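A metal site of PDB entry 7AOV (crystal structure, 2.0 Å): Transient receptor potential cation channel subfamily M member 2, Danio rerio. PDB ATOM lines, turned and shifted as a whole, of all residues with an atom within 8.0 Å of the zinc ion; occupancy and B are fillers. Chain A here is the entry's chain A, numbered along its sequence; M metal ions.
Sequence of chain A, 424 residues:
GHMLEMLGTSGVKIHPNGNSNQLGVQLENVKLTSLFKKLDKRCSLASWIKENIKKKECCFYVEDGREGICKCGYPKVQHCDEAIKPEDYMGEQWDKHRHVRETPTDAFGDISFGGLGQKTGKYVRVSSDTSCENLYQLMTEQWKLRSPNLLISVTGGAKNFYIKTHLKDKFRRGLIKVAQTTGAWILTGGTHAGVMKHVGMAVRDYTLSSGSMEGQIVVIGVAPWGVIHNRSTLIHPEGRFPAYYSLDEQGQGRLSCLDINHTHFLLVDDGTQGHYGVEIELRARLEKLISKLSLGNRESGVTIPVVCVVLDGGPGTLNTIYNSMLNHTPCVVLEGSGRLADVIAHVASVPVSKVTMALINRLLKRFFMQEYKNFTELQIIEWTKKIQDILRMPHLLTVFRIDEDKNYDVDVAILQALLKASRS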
ATOM      1  N   GLU A  57      14.755  -6.501  15.168  1.00  0.00           N
ATOM      2  CA  GLU A  57      15.450  -7.348  16.128  1.00  0.00           C
ATOM      3  C   GLU A  57      16.422  -8.260  15.414  1.00  0.00           C
ATOM      4  O   GLU A  57      16.086  -8.853  14.388  1.00  0.00           O
ATOM      5  CB  GLU A  57      14.488  -8.206  16.921  1.00  0.00           C
ATOM      6  CG  GLU A  57      13.594  -7.422  17.815  1.00  0.00           C
ATOM      7  CD  GLU A  57      12.761  -8.307  18.681  1.00  0.00           C
ATOM      8  OE1 GLU A  57      12.852  -8.163  19.920  1.00  0.00           O
ATOM      9  OE2 GLU A  57      12.037  -9.168  18.129  1.00  0.00           O
ATOM     10  N   CYS A  58      17.613  -8.404  16.007  1.00  0.00           N
ATOM     11  CA  CYS A  58      18.594  -9.390  15.570  1.00  0.00           C
ATOM     12  C   CYS A  58      18.065 -10.801  15.671  1.00  0.00           C
ATOM     13  O   CYS A  58      17.483 -11.199  16.689  1.00  0.00           O
ATOM     14  CB  CYS A  58      19.870  -9.230  16.392  1.00  0.00           C
ATOM     15  SG  CYS A  58      21.208 -10.393  16.052  1.00  0.00           S
ATOM     16  N   CYS A  59      18.289 -11.591  14.611  1.00  0.00           N
ATOM     17  CA  CYS A  59      17.869 -12.981  14.574  1.00  0.00           C
ATOM     18  C   CYS A  59      19.050 -13.923  14.375  1.00  0.00           C
ATOM     19  O   CYS A  59      18.862 -15.050  13.907  1.00  0.00           O
ATOM     20  CB  CYS A  59      16.824 -13.193  13.466  1.00  0.00           C
ATOM     21  SG  CYS A  59      15.195 -12.452  13.826  1.00  0.00           S
ATOM     22  N   PHE A  60      20.258 -13.485  14.738  1.00  0.00           N
ATOM     23  CA  PHE A  60      21.465 -14.294  14.533  1.00  0.00           C
ATOM     24  C   PHE A  60      22.501 -13.800  15.549  1.00  0.00           C
ATOM     25  O   PHE A  60      23.208 -12.821  15.289  1.00  0.00           O
ATOM     26  CB  PHE A  60      21.967 -14.155  13.109  1.00  0.00           C
ATOM     27  CG  PHE A  60      23.090 -15.088  12.762  1.00  0.00           C
ATOM     28  CD1 PHE A  60      23.230 -16.307  13.411  1.00  0.00           C
ATOM     29  CD2 PHE A  60      23.992 -14.757  11.766  1.00  0.00           C
ATOM     30  CE1 PHE A  60      24.250 -17.167  13.073  1.00  0.00           C
ATOM     31  CE2 PHE A  60      25.024 -15.619  11.422  1.00  0.00           C
ATOM     32  CZ  PHE A  60      25.150 -16.820  12.070  1.00  0.00           C
ATOM     33  N   TYR A  61      22.588 -14.479  16.694  1.00  0.00           N
ATOM     34  CA  TYR A  61      23.509 -14.088  17.753  1.00  0.00           C
ATOM     35  C   TYR A  61      24.919 -14.501  17.380  1.00  0.00           C
ATOM     36  O   TYR A  61      25.222 -15.702  17.302  1.00  0.00           O
ATOM     37  CB  TYR A  61      23.111 -14.712  19.094  1.00  0.00           C
ATOM     38  CG  TYR A  61      24.145 -14.408  20.167  1.00  0.00           C
ATOM     39  CD1 TYR A  61      24.109 -13.211  20.850  1.00  0.00           C
ATOM     40  CD2 TYR A  61      25.167 -15.304  20.477  1.00  0.00           C
ATOM     41  CE1 TYR A  61      25.049 -12.901  21.815  1.00  0.00           C
ATOM     42  CE2 TYR A  61      26.109 -15.010  21.449  1.00  0.00           C
ATOM     43  CZ  TYR A  61      26.035 -13.802  22.119  1.00  0.00           C
ATOM     44  OH  TYR A  61      26.963 -13.496  23.077  1.00  0.00           O
ATOM     45  N   VAL A  62      25.808 -13.538  17.151  1.00  0.00           N
ATOM     46  CA  VAL A  62      27.193 -13.834  16.801  1.00  0.00           C
ATOM     47  C   VAL A  62      28.089 -12.841  17.526  1.00  0.00           C
ATOM     48  O   VAL A  62      27.933 -11.617  17.381  1.00  0.00           O
ATOM     49  CB  VAL A  62      27.440 -13.783  15.283  1.00  0.00           C
ATOM     50  CG1 VAL A  62      28.890 -14.133  14.969  1.00  0.00           C
ATOM     51  CG2 VAL A  62      26.471 -14.732  14.527  1.00  0.00           C
ATOM     52  N   GLU A  63      29.034 -13.353  18.287  1.00  0.00           N
ATOM     53  CA  GLU A  63      29.844 -12.473  19.099  1.00  0.00           C
ATOM     54  C   GLU A  63      30.884 -11.768  18.239  1.00  0.00           C
ATOM     55  O   GLU A  63      31.171 -12.157  17.098  1.00  0.00           O
ATOM     56  CB  GLU A  63      30.517 -13.255  20.215  1.00  0.00           C
ATOM     57  CG  GLU A  63      29.551 -13.510  21.330  1.00  0.00           C
ATOM     58  CD  GLU A  63      29.990 -14.643  22.240  1.00  0.00           C
ATOM     59  OE1 GLU A  63      31.038 -15.252  21.943  1.00  0.00           O
ATOM     60  OE2 GLU A  63      29.306 -14.883  23.258  1.00  0.00           O
ATOM     61  N   ILE A  69      28.254 -10.462  24.199  1.00  0.00           N
ATOM     62  CA  ILE A  69      27.731  -9.355  23.413  1.00  0.00           C
ATOM     63  C   ILE A  69      27.798  -9.729  21.929  1.00  0.00           C
ATOM     64  O   ILE A  69      28.875 -10.051  21.422  1.00  0.00           O
ATOM     65  CB  ILE A  69      28.512  -8.053  23.655  1.00  0.00           C
ATOM     66  CG1 ILE A  69      28.669  -7.775  25.155  1.00  0.00           C
ATOM     67  CG2 ILE A  69      27.796  -6.902  22.966  1.00  0.00           C
ATOM     68  CD1 ILE A  69      27.340  -7.648  25.889  1.00  0.00           C
ATOM     69  N   CYS A  70      26.652  -9.628  21.264  1.00  0.00           N
ATOM     70  CA  CYS A  70      26.500  -9.874  19.843  1.00  0.00           C
ATOM     71  C   CYS A  70      27.092  -8.744  19.009  1.00  0.00           C
ATOM     72  O   CYS A  70      27.309  -7.622  19.489  1.00  0.00           O
ATOM     73  CB  CYS A  70      25.019 -10.025  19.499  1.00  0.00           C
ATOM     74  SG  CYS A  70      24.663 -10.462  17.783  1.00  0.00           S
ATOM     75  N   LYS A  71      27.349  -9.039  17.745  1.00  0.00           N
ATOM     76  CA  LYS A  71      27.721  -7.970  16.829  1.00  0.00           C
ATOM     77  C   LYS A  71      26.642  -6.885  16.740  1.00  0.00           C
ATOM     78  O   LYS A  71      26.976  -5.732  16.477  1.00  0.00           O
ATOM     79  CB  LYS A  71      28.009  -8.544  15.430  1.00  0.00           C
ATOM     80  CG  LYS A  71      28.724  -7.561  14.506  1.00  0.00           C
ATOM     81  CD  LYS A  71      29.338  -8.250  13.299  1.00  0.00           C
ATOM     82  CE  LYS A  71      30.829  -8.100  13.285  1.00  0.00           C
ATOM     83  NZ  LYS A  71      31.260  -6.847  12.630  1.00  0.00           N
ATOM     84  N   CYS A  72      25.369  -7.218  16.957  1.00  0.00           N
ATOM     85  CA  CYS A  72      24.342  -6.182  17.003  1.00  0.00           C
ATOM     86  C   CYS A  72      24.487  -5.257  18.210  1.00  0.00           C
ATOM     87  O   CYS A  72      23.840  -4.210  18.259  1.00  0.00           O
ATOM     88  CB  CYS A  72      22.911  -6.792  16.967  1.00  0.00           C
ATOM     89  SG  CYS A  72      22.432  -7.648  18.521  1.00  0.00           S
ATOM     90  N   GLY A  73      25.330  -5.598  19.192  1.00  0.00           N
ATOM     91  CA  GLY A  73      25.499  -4.758  20.362  1.00  0.00           C
ATOM     92  C   GLY A  73      24.649  -5.145  21.558  1.00  0.00           C
ATOM     93  O   GLY A  73      24.885  -4.631  22.664  1.00  0.00           O
ATOM     94  N   TYR A  74      23.661  -6.054  21.384  1.00  0.00           N
ATOM     95  CA  TYR A  74      22.861  -6.440  22.534  1.00  0.00           C
ATOM     96  C   TYR A  74      23.468  -7.664  23.221  1.00  0.00           C
ATOM     97  O   TYR A  74      24.052  -8.534  22.549  1.00  0.00           O
ATOM     98  CB  TYR A  74      21.415  -6.766  22.109  1.00  0.00           C
ATOM     99  CG  TYR A  74      20.527  -5.548  21.851  1.00  0.00           C
ATOM    100  CD1 TYR A  74      19.887  -4.882  22.903  1.00  0.00           C
ATOM    101  CD2 TYR A  74      20.334  -5.078  20.564  1.00  0.00           C
ATOM    102  CE1 TYR A  74      19.081  -3.771  22.650  1.00  0.00           C
ATOM    103  CE2 TYR A  74      19.538  -3.977  20.300  1.00  0.00           C
ATOM    104  CZ  TYR A  74      18.907  -3.331  21.362  1.00  0.00           C
ATOM    105  OH  TYR A  74      18.115  -2.237  21.111  1.00  0.00           O
ATOM    106  N   PRO A  75      23.317  -7.776  24.538  1.00  0.00           N
ATOM    107  CA  PRO A  75      23.724  -9.002  25.225  1.00  0.00           C
ATOM    108  C   PRO A  75      22.928 -10.204  24.734  1.00  0.00           C
ATOM    109  O   PRO A  75      21.816 -10.084  24.225  1.00  0.00           O
ATOM    110  CB  PRO A  75      23.405  -8.709  26.698  1.00  0.00           C
ATOM    111  CG  PRO A  75      23.260  -7.227  26.792  1.00  0.00           C
ATOM    112  CD  PRO A  75      22.742  -6.778  25.455  1.00  0.00           C
ATOM    113  N   LYS A  76      23.534 -11.381  24.946  1.00  0.00           N
ATOM    114  CA  LYS A  76      22.918 -12.638  24.543  1.00  0.00           C
ATOM    115  C   LYS A  76      21.554 -12.836  25.200  1.00  0.00           C
ATOM    116  O   LYS A  76      20.602 -13.279  24.554  1.00  0.00           O
ATOM    117  CB  LYS A  76      23.847 -13.802  24.880  1.00  0.00           C
ATOM    118  CG  LYS A  76      23.268 -15.171  24.585  1.00  0.00           C
ATOM    119  CD  LYS A  76      24.201 -16.309  25.035  1.00  0.00           C
ATOM    120  CE  LYS A  76      24.777 -17.078  23.856  1.00  0.00           C
ATOM    121  NZ  LYS A  76      25.381 -18.395  24.219  1.00  0.00           N
ATOM    122  N   GLN A  78      19.401 -10.767  25.983  1.00  0.00           N
ATOM    123  CA  GLN A  78      18.389  -9.925  25.379  1.00  0.00           C
ATOM    124  C   GLN A  78      18.054 -10.342  23.951  1.00  0.00           C
ATOM    125  O   GLN A  78      17.457  -9.559  23.220  1.00  0.00           O
ATOM    126  CB  GLN A  78      18.827  -8.459  25.412  1.00  0.00           C
ATOM    127  CG  GLN A  78      18.639  -7.834  26.768  1.00  0.00           C
ATOM    128  CD  GLN A  78      19.361  -6.499  26.913  1.00  0.00           C
ATOM    129  OE1 GLN A  78      20.275  -6.365  27.724  1.00  0.00           O
ATOM    130  NE2 GLN A  78      18.936  -5.506  26.139  1.00  0.00           N
ATOM    131  N   HIS A  79      18.417 -11.549  23.535  1.00  0.00           N
ATOM    132  CA  HIS A  79      18.078 -12.026  22.213  1.00  0.00           C
ATOM    133  C   HIS A  79      16.921 -13.000  22.295  1.00  0.00           C
ATOM    134  O   HIS A  79      16.742 -13.676  23.311  1.00  0.00           O
ATOM    135  CB  HIS A  79      19.260 -12.739  21.548  1.00  0.00           C
ATOM    136  CG  HIS A  79      20.277 -11.815  20.969  1.00  0.00           C
ATOM    137  ND1 HIS A  79      21.157 -11.087  21.745  1.00  0.00           N
ATOM    138  CD2 HIS A  79      20.572 -11.505  19.683  1.00  0.00           C
ATOM    139  CE1 HIS A  79      21.945 -10.374  20.957  1.00  0.00           C
ATOM    140  NE2 HIS A  79      21.616 -10.618  19.707  1.00  0.00           N
ATOM    141  N   CYS A  80      16.157 -13.090  21.213  1.00  0.00           N
ATOM    142  CA  CYS A  80      15.158 -14.143  21.128  1.00  0.00           C
ATOM    143  C   CYS A  80      15.866 -15.487  21.009  1.00  0.00           C
ATOM    144  O   CYS A  80      17.019 -15.582  20.579  1.00  0.00           O
ATOM    145  CB  CYS A  80      14.223 -13.914  19.937  1.00  0.00           C
ATOM    146  SG  CYS A  80      15.001 -13.586  18.352  1.00  0.00           S
ATOM    147  N   ALA A  83      17.311 -16.516  17.694  1.00  0.00           N
ATOM    148  CA  ALA A  83      18.602 -15.981  17.306  1.00  0.00           C
ATOM    149  C   ALA A  83      19.753 -16.909  17.676  1.00  0.00           C
ATOM    150  O   ALA A  83      20.855 -16.766  17.134  1.00  0.00           O
ATOM    151  CB  ALA A  83      18.830 -14.598  17.946  1.00  0.00           C
ATOM    152  N   ILE A  84      19.531 -17.857  18.581  1.00  0.00           N
ATOM    153  CA  ILE A  84      20.620 -18.734  19.018  1.00  0.00           C
ATOM    154  C   ILE A  84      20.757 -19.871  18.023  1.00  0.00           C
ATOM    155  O   ILE A  84      19.851 -20.688  17.855  1.00  0.00           O
ATOM    156  CB  ILE A  84      20.397 -19.246  20.447  1.00  0.00           C
ATOM    157  CG1 ILE A  84      19.978 -18.094  21.354  1.00  0.00           C
ATOM    158  CG2 ILE A  84      21.669 -19.892  20.965  1.00  0.00           C
ATOM    159  CD1 ILE A  84      20.903 -16.873  21.319  1.00  0.00           C
ATOM    160  N   TRP A  94      28.025 -12.231  10.385  1.00  0.00           N
ATOM    161  CA  TRP A  94      26.882 -11.408  10.758  1.00  0.00           C
ATOM    162  C   TRP A  94      26.814 -10.151   9.892  1.00  0.00           C
ATOM    163  O   TRP A  94      27.837  -9.542   9.553  1.00  0.00           O
ATOM    164  CB  TRP A  94      26.986 -11.026  12.231  1.00  0.00           C
ATOM    165  CG  TRP A  94      25.722 -10.456  12.795  1.00  0.00           C
ATOM    166  CD1 TRP A  94      24.714 -11.127  13.406  1.00  0.00           C
ATOM    167  CD2 TRP A  94      25.315  -9.069  12.767  1.00  0.00           C
ATOM    168  NE1 TRP A  94      23.698 -10.268  13.768  1.00  0.00           N
ATOM    169  CE2 TRP A  94      24.048  -8.995  13.388  1.00  0.00           C
ATOM    170  CE3 TRP A  94      25.893  -7.885  12.282  1.00  0.00           C
ATOM    171  CZ2 TRP A  94      23.363  -7.785  13.547  1.00  0.00           C
ATOM    172  CZ3 TRP A  94      25.200  -6.686  12.445  1.00  0.00           C
ATOM    173  CH2 TRP A  94      23.957  -6.650  13.078  1.00  0.00           C
ATOM    174  N   HIS A  99      20.432 -10.306   8.780  1.00  0.00           N
ATOM    175  CA  HIS A  99      20.176 -11.053  10.013  1.00  0.00           C
ATOM    176  C   HIS A  99      19.372 -10.282  11.056  1.00  0.00           C
ATOM    177  O   HIS A  99      19.308 -10.709  12.218  1.00  0.00           O
ATOM    178  CB  HIS A  99      21.495 -11.532  10.634  1.00  0.00           C
ATOM    179  CG  HIS A  99      22.282 -12.460   9.764  1.00  0.00           C
ATOM    180  ND1 HIS A  99      23.551 -12.161   9.297  1.00  0.00           N
ATOM    181  CD2 HIS A  99      21.983 -13.680   9.263  1.00  0.00           C
ATOM    182  CE1 HIS A  99      24.002 -13.160   8.562  1.00  0.00           C
ATOM    183  NE2 HIS A  99      23.056 -14.097   8.512  1.00  0.00           N
ATOM    184  N   VAL A 100      18.798  -9.144  10.699  1.00  0.00           N
ATOM    185  CA  VAL A 100      17.785  -8.507  11.531  1.00  0.00           C
ATOM    186  C   VAL A 100      16.470  -8.607  10.788  1.00  0.00           C
ATOM    187  O   VAL A 100      16.428  -8.595   9.549  1.00  0.00           O
ATOM    188  CB  VAL A 100      18.105  -7.030  11.866  1.00  0.00           C
ATOM    189  CG1 VAL A 100      19.509  -6.910  12.416  1.00  0.00           C
ATOM    190  CG2 VAL A 100      17.956  -6.170  10.666  1.00  0.00           C
ATOM    191  N   GLY A 271      17.956  -2.520  14.699  1.00  0.00           N
ATOM    192  CA  GLY A 271      18.219  -3.791  15.354  1.00  0.00           C
ATOM    193  C   GLY A 271      19.474  -3.833  16.199  1.00  0.00           C
ATOM    194  O   GLY A 271      19.752  -4.873  16.825  1.00  0.00           O
ATOM    195  N   THR A 272      20.225  -2.751  16.260  1.00  0.00           N
ATOM    196  CA  THR A 272      21.513  -2.731  16.945  1.00  0.00           C
ATOM    197  C   THR A 272      21.446  -1.762  18.115  1.00  0.00           C
ATOM    198  O   THR A 272      20.545  -0.926  18.204  1.00  0.00           O
ATOM    199  CB  THR A 272      22.647  -2.327  15.972  1.00  0.00           C
ATOM    200  OG1 THR A 272      22.511  -0.939  15.658  1.00  0.00           O
ATOM    201  CG2 THR A 272      22.588  -3.156  14.684  1.00  0.00           C
HETATM  202 ZN    ZN M   1      22.483  -9.878  17.895  1.00  0.00          ZN
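SG of Cys 58 lies close to O of Phe 60 (3.2 Å). SG of Cys 58 sits close to NE1 of Trp 94, 3.4 Å away. A ring nitrogen (ND1) of His 79 sits at hydrogen-bond distance from the backbone carbonyl oxygen of Pro 75, 2.8 Å away. The side-chain sulfur (SG) of Cys 70 sits close to the backbone carbonyl oxygen (O) of Phe 60 (3.7 Å). The backbone NH (N) of Tyr 74 lies close to the side-chain sulfur (SG) of Cys 72, 3.5 Å away. O of Phe 60 sits close to NE1 of Trp 94 (3.0 Å). The backbone NH (N) of Val 62 lies close to the side-chain sulfur (SG) of Cys 70.
Phe 60 touches the zinc ion. Five residues have an atom within 4 Å of the zinc ion: Cys 58, Phe 60, Cys 70, Cys 72 and His 79. The nearest printed residue that does not touch the zinc ion is Trp 94 (4.3 Å).
The zinc ion is bound by a ring nitrogen (NE2) of His 79 (2.1 Å), the side-chain sulfur (SG) of Cys 70 (2.3 Å), the side-chain sulfur (SG) of Cys 58 (2.3 Å) and the side-chain sulfur (SG) of Cys 72 (2.3 Å).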
